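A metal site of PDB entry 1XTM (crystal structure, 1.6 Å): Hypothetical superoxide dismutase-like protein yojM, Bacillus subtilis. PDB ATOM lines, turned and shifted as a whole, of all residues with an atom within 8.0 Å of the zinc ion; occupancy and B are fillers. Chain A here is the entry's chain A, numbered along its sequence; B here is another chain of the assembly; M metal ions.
Within 4 Å of the zinc ion: His 50 of chain A, Asp 116 of chain A, His 50 of chain B and Asp 116 of chain B.
The nearest printed residue that does not touch the zinc ion is Ser 52 of chain A (4.2 Å).
The zinc ion is bound by OD1 of Asp 116 of chain B (1.9 Å), OD1 of Asp 116 of chain A (2.0 Å), NE2 of His 50 of chain B (2.2 Å) and NE2 of His 50 of chain A (2.2 Å).
The zinc ion has four donor atoms within binding distance.
OG of Ser 52 of chain A sits close to OD2 of Asp 116 of chain A, at 3.5 Å.
OD1 of Asp 116 of chain B lies close to OG of Ser 52 of chain B (3.5 Å).
OG of Ser 52 of chain A is in hydrogen-bond range of OD2 of Asp 116 of chain B, 2.7 Å away.
OG of Ser 52 of chain B lies within hydrogen-bond range of OD2 of Asp 116 of chain A (2.8 Å).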
ATOM      1  N   PHE A  36      32.429  -2.381 -14.182  1.00  0.00           N
ATOM      2  CA  PHE A  36      33.748  -2.941 -14.013  1.00  0.00           C
ATOM      3  C   PHE A  36      33.784  -4.408 -14.372  1.00  0.00           C
ATOM      4  O   PHE A  36      32.728  -5.035 -14.526  1.00  0.00           O
ATOM      5  CB  PHE A  36      34.254  -2.702 -12.575  1.00  0.00           C
ATOM      6  CG  PHE A  36      33.554  -3.545 -11.503  1.00  0.00           C
ATOM      7  CD1 PHE A  36      32.404  -3.065 -10.862  1.00  0.00           C
ATOM      8  CD2 PHE A  36      34.063  -4.794 -11.124  1.00  0.00           C
ATOM      9  CE1 PHE A  36      31.757  -3.855  -9.847  1.00  0.00           C
ATOM     10  CE2 PHE A  36      33.442  -5.575 -10.118  1.00  0.00           C
ATOM     11  CZ  PHE A  36      32.296  -5.093  -9.486  1.00  0.00           C
ATOM     12  N   HIS A  50      33.950 -11.779 -13.729  1.00  0.00           N
ATOM     13  CA  HIS A  50      32.868 -11.026 -13.079  1.00  0.00           C
ATOM     14  C   HIS A  50      32.619  -9.694 -13.800  1.00  0.00           C
ATOM     15  O   HIS A  50      33.447  -8.789 -13.751  1.00  0.00           O
ATOM     16  CB  HIS A  50      33.237 -10.808 -11.578  1.00  0.00           C
ATOM     17  CG  HIS A  50      32.222 -10.035 -10.780  1.00  0.00           C
ATOM     18  ND1 HIS A  50      32.574  -9.309  -9.664  1.00  0.00           N
ATOM     19  CD2 HIS A  50      30.872  -9.908 -10.894  1.00  0.00           C
ATOM     20  CE1 HIS A  50      31.502  -8.751  -9.141  1.00  0.00           C
ATOM     21  NE2 HIS A  50      30.458  -9.088  -9.880  1.00  0.00           N
ATOM     22  N   ILE A  51      31.482  -9.555 -14.482  1.00  0.00           N
ATOM     23  CA  ILE A  51      31.122  -8.282 -15.115  1.00  0.00           C
ATOM     24  C   ILE A  51      29.896  -7.667 -14.479  1.00  0.00           C
ATOM     25  O   ILE A  51      28.867  -8.323 -14.324  1.00  0.00           O
ATOM     26  CB  ILE A  51      30.933  -8.397 -16.660  1.00  0.00           C
ATOM     27  CG1 ILE A  51      30.224  -7.155 -17.193  1.00  0.00           C
ATOM     28  CG2 ILE A  51      30.176  -9.697 -17.043  1.00  0.00           C
ATOM     29  CD1 ILE A  51      30.213  -7.042 -18.706  1.00  0.00           C
ATOM     30  N   SER A  52      30.010  -6.401 -14.098  1.00  0.00           N
ATOM     31  CA  SER A  52      28.910  -5.662 -13.501  1.00  0.00           C
ATOM     32  C   SER A  52      28.782  -4.288 -14.158  1.00  0.00           C
ATOM     33  O   SER A  52      29.574  -3.373 -13.871  1.00  0.00           O
ATOM     34  CB  SER A  52      29.090  -5.559 -11.972  1.00  0.00           C
ATOM     35  OG  SER A  52      27.885  -5.173 -11.335  1.00  0.00           O
ATOM     36  N   ALA A  53      27.780  -4.156 -15.038  1.00  0.00           N
ATOM     37  CA  ALA A  53      27.629  -2.964 -15.898  1.00  0.00           C
ATOM     38  C   ALA A  53      26.247  -2.351 -15.831  1.00  0.00           C
ATOM     39  O   ALA A  53      25.300  -2.984 -15.370  1.00  0.00           O
ATOM     40  CB  ALA A  53      27.948  -3.315 -17.333  1.00  0.00           C
ATOM     41  N   VAL A 115      23.662  -5.380 -16.041  1.00  0.00           N
ATOM     42  CA  VAL A 115      24.063  -6.778 -16.075  1.00  0.00           C
ATOM     43  C   VAL A 115      25.068  -7.028 -14.954  1.00  0.00           C
ATOM     44  O   VAL A 115      25.956  -6.215 -14.734  1.00  0.00           O
ATOM     45  CB  VAL A 115      24.635  -7.175 -17.465  1.00  0.00           C
ATOM     46  CG1 VAL A 115      25.883  -6.366 -17.824  1.00  0.00           C
ATOM     47  CG2 VAL A 115      24.925  -8.646 -17.554  1.00  0.00           C
ATOM     48  N   ASP A 116      24.927  -8.146 -14.236  1.00  0.00           N
ATOM     49  CA  ASP A 116      25.799  -8.419 -13.083  1.00  0.00           C
ATOM     50  C   ASP A 116      25.984  -9.940 -12.917  1.00  0.00           C
ATOM     51  O   ASP A 116      25.201 -10.582 -12.210  1.00  0.00           O
ATOM     52  CB  ASP A 116      25.219  -7.778 -11.827  1.00  0.00           C
ATOM     53  CG  ASP A 116      26.160  -7.907 -10.623  1.00  0.00           C
ATOM     54  OD1 ASP A 116      27.208  -8.577 -10.729  1.00  0.00           O
ATOM     55  OD2 ASP A 116      25.882  -7.370  -9.519  1.00  0.00           O
ATOM     56  N   VAL A 117      26.992 -10.479 -13.612  1.00  0.00           N
ATOM     57  CA  VAL A 117      27.203 -11.942 -13.708  1.00  0.00           C
ATOM     58  C   VAL A 117      28.673 -12.360 -13.686  1.00  0.00           C
ATOM     59  O   VAL A 117      29.570 -11.540 -13.852  1.00  0.00           O
ATOM     60  CB  VAL A 117      26.553 -12.590 -14.990  1.00  0.00           C
ATOM     61  CG1 VAL A 117      25.039 -12.254 -15.087  1.00  0.00           C
ATOM     62  CG2 VAL A 117      27.364 -12.227 -16.309  1.00  0.00           C
ATOM     63  N   ILE A 118      28.893 -13.646 -13.466  1.00  0.00           N
ATOM     64  CA  ILE A 118      30.206 -14.227 -13.607  1.00  0.00           C
ATOM     65  C   ILE A 118      30.123 -15.255 -14.727  1.00  0.00           C
ATOM     66  O   ILE A 118      29.290 -16.162 -14.682  1.00  0.00           O
ATOM     67  CB  ILE A 118      30.714 -14.864 -12.288  1.00  0.00           C
ATOM     68  CG1 ILE A 118      30.747 -13.825 -11.152  1.00  0.00           C
ATOM     69  CG2 ILE A 118      32.112 -15.471 -12.477  1.00  0.00           C
ATOM     70  CD1 ILE A 118      29.446 -13.632 -10.401  1.00  0.00           C
ATOM     71  N   PHE B  36      20.821  -8.942  -4.231  1.00  0.00           N
ATOM     72  CA  PHE B  36      20.631 -10.382  -4.346  1.00  0.00           C
ATOM     73  C   PHE B  36      21.890 -11.106  -4.012  1.00  0.00           C
ATOM     74  O   PHE B  36      22.990 -10.529  -3.981  1.00  0.00           O
ATOM     75  CB  PHE B  36      20.205 -10.859  -5.762  1.00  0.00           C
ATOM     76  CG  PHE B  36      21.274 -10.667  -6.839  1.00  0.00           C
ATOM     77  CD1 PHE B  36      21.408  -9.422  -7.505  1.00  0.00           C
ATOM     78  CD2 PHE B  36      22.162 -11.678  -7.162  1.00  0.00           C
ATOM     79  CE1 PHE B  36      22.408  -9.230  -8.456  1.00  0.00           C
ATOM     80  CE2 PHE B  36      23.175 -11.476  -8.129  1.00  0.00           C
ATOM     81  CZ  PHE B  36      23.292 -10.256  -8.773  1.00  0.00           C
ATOM     82  N   HIS B  50      27.981 -15.097  -4.697  1.00  0.00           N
ATOM     83  CA  HIS B  50      28.032 -13.805  -5.354  1.00  0.00           C
ATOM     84  C   HIS B  50      27.033 -12.896  -4.646  1.00  0.00           C
ATOM     85  O   HIS B  50      25.828 -13.182  -4.668  1.00  0.00           O
ATOM     86  CB  HIS B  50      27.676 -13.996  -6.846  1.00  0.00           C
ATOM     87  CG  HIS B  50      27.569 -12.722  -7.632  1.00  0.00           C
ATOM     88  ND1 HIS B  50      26.794 -12.621  -8.778  1.00  0.00           N
ATOM     89  CD2 HIS B  50      28.186 -11.514  -7.491  1.00  0.00           C
ATOM     90  CE1 HIS B  50      26.915 -11.401  -9.290  1.00  0.00           C
ATOM     91  NE2 HIS B  50      27.739 -10.710  -8.509  1.00  0.00           N
ATOM     92  N   ILE B  51      27.524 -11.823  -4.002  1.00  0.00           N
ATOM     93  CA  ILE B  51      26.612 -10.914  -3.283  1.00  0.00           C
ATOM     94  C   ILE B  51      26.687  -9.553  -3.919  1.00  0.00           C
ATOM     95  O   ILE B  51      27.774  -8.964  -4.053  1.00  0.00           O
ATOM     96  CB  ILE B  51      26.905 -10.854  -1.740  1.00  0.00           C
ATOM     97  CG1 ILE B  51      26.080  -9.707  -1.065  1.00  0.00           C
ATOM     98  CG2 ILE B  51      28.374 -10.683  -1.508  1.00  0.00           C
ATOM     99  CD1 ILE B  51      25.739  -9.906   0.407  1.00  0.00           C
ATOM    100  N   SER B  52      25.524  -9.047  -4.351  1.00  0.00           N
ATOM    101  CA  SER B  52      25.509  -7.705  -4.928  1.00  0.00           C
ATOM    102  C   SER B  52      24.403  -6.915  -4.248  1.00  0.00           C
ATOM    103  O   SER B  52      23.219  -7.096  -4.558  1.00  0.00           O
ATOM    104  CB  SER B  52      25.377  -7.707  -6.453  1.00  0.00           C
ATOM    105  OG  SER B  52      25.633  -6.401  -6.953  1.00  0.00           O
ATOM    106  N   ALA B  53      24.787  -6.067  -3.305  1.00  0.00           N
ATOM    107  CA  ALA B  53      23.845  -5.378  -2.428  1.00  0.00           C
ATOM    108  C   ALA B  53      24.102  -3.900  -2.530  1.00  0.00           C
ATOM    109  O   ALA B  53      25.140  -3.466  -3.035  1.00  0.00           O
ATOM    110  CB  ALA B  53      23.978  -5.801  -0.976  1.00  0.00           C
ATOM    111  N   VAL B 115      28.031  -3.254  -2.133  1.00  0.00           N
ATOM    112  CA  VAL B 115      29.010  -4.357  -2.145  1.00  0.00           C
ATOM    113  C   VAL B 115      28.659  -5.211  -3.359  1.00  0.00           C
ATOM    114  O   VAL B 115      27.478  -5.436  -3.621  1.00  0.00           O
ATOM    115  CB  VAL B 115      29.076  -5.208  -0.803  1.00  0.00           C
ATOM    116  CG1 VAL B 115      27.710  -5.587  -0.284  1.00  0.00           C
ATOM    117  CG2 VAL B 115      29.962  -6.468  -0.965  1.00  0.00           C
ATOM    118  N   ASP B 116      29.670  -5.619  -4.106  1.00  0.00           N
ATOM    119  CA  ASP B 116      29.444  -6.471  -5.272  1.00  0.00           C
ATOM    120  C   ASP B 116      30.654  -7.366  -5.474  1.00  0.00           C
ATOM    121  O   ASP B 116      31.617  -6.977  -6.146  1.00  0.00           O
ATOM    122  CB  ASP B 116      29.165  -5.606  -6.509  1.00  0.00           C
ATOM    123  CG  ASP B 116      28.813  -6.418  -7.716  1.00  0.00           C
ATOM    124  OD1 ASP B 116      28.765  -7.677  -7.648  1.00  0.00           O
ATOM    125  OD2 ASP B 116      28.616  -5.884  -8.848  1.00  0.00           O
ATOM    126  N   VAL B 117      30.581  -8.568  -4.886  1.00  0.00           N
ATOM    127  CA  VAL B 117      31.780  -9.410  -4.671  1.00  0.00           C
ATOM    128  C   VAL B 117      31.416 -10.878  -4.728  1.00  0.00           C
ATOM    129  O   VAL B 117      30.233 -11.244  -4.614  1.00  0.00           O
ATOM    130  CB  VAL B 117      32.528  -9.150  -3.289  1.00  0.00           C
ATOM    131  CG1 VAL B 117      32.952  -7.669  -3.088  1.00  0.00           C
ATOM    132  CG2 VAL B 117      31.702  -9.648  -2.108  1.00  0.00           C
ATOM    133  N   ILE B 118      32.438 -11.734  -4.887  1.00  0.00           N
ATOM    134  CA  ILE B 118      32.233 -13.179  -4.802  1.00  0.00           C
ATOM    135  C   ILE B 118      33.144 -13.704  -3.721  1.00  0.00           C
ATOM    136  O   ILE B 118      34.377 -13.518  -3.783  1.00  0.00           O
ATOM    137  CB  ILE B 118      32.533 -13.890  -6.145  1.00  0.00           C
ATOM    138  CG1 ILE B 118      31.614 -13.408  -7.269  1.00  0.00           C
ATOM    139  CG2 ILE B 118      32.484 -15.405  -5.959  1.00  0.00           C
ATOM    140  CD1 ILE B 118      32.195 -12.222  -8.045  1.00  0.00           C
HETATM  141 ZN    ZN M   1      28.409  -8.762  -9.196  1.00  0.00          ZN
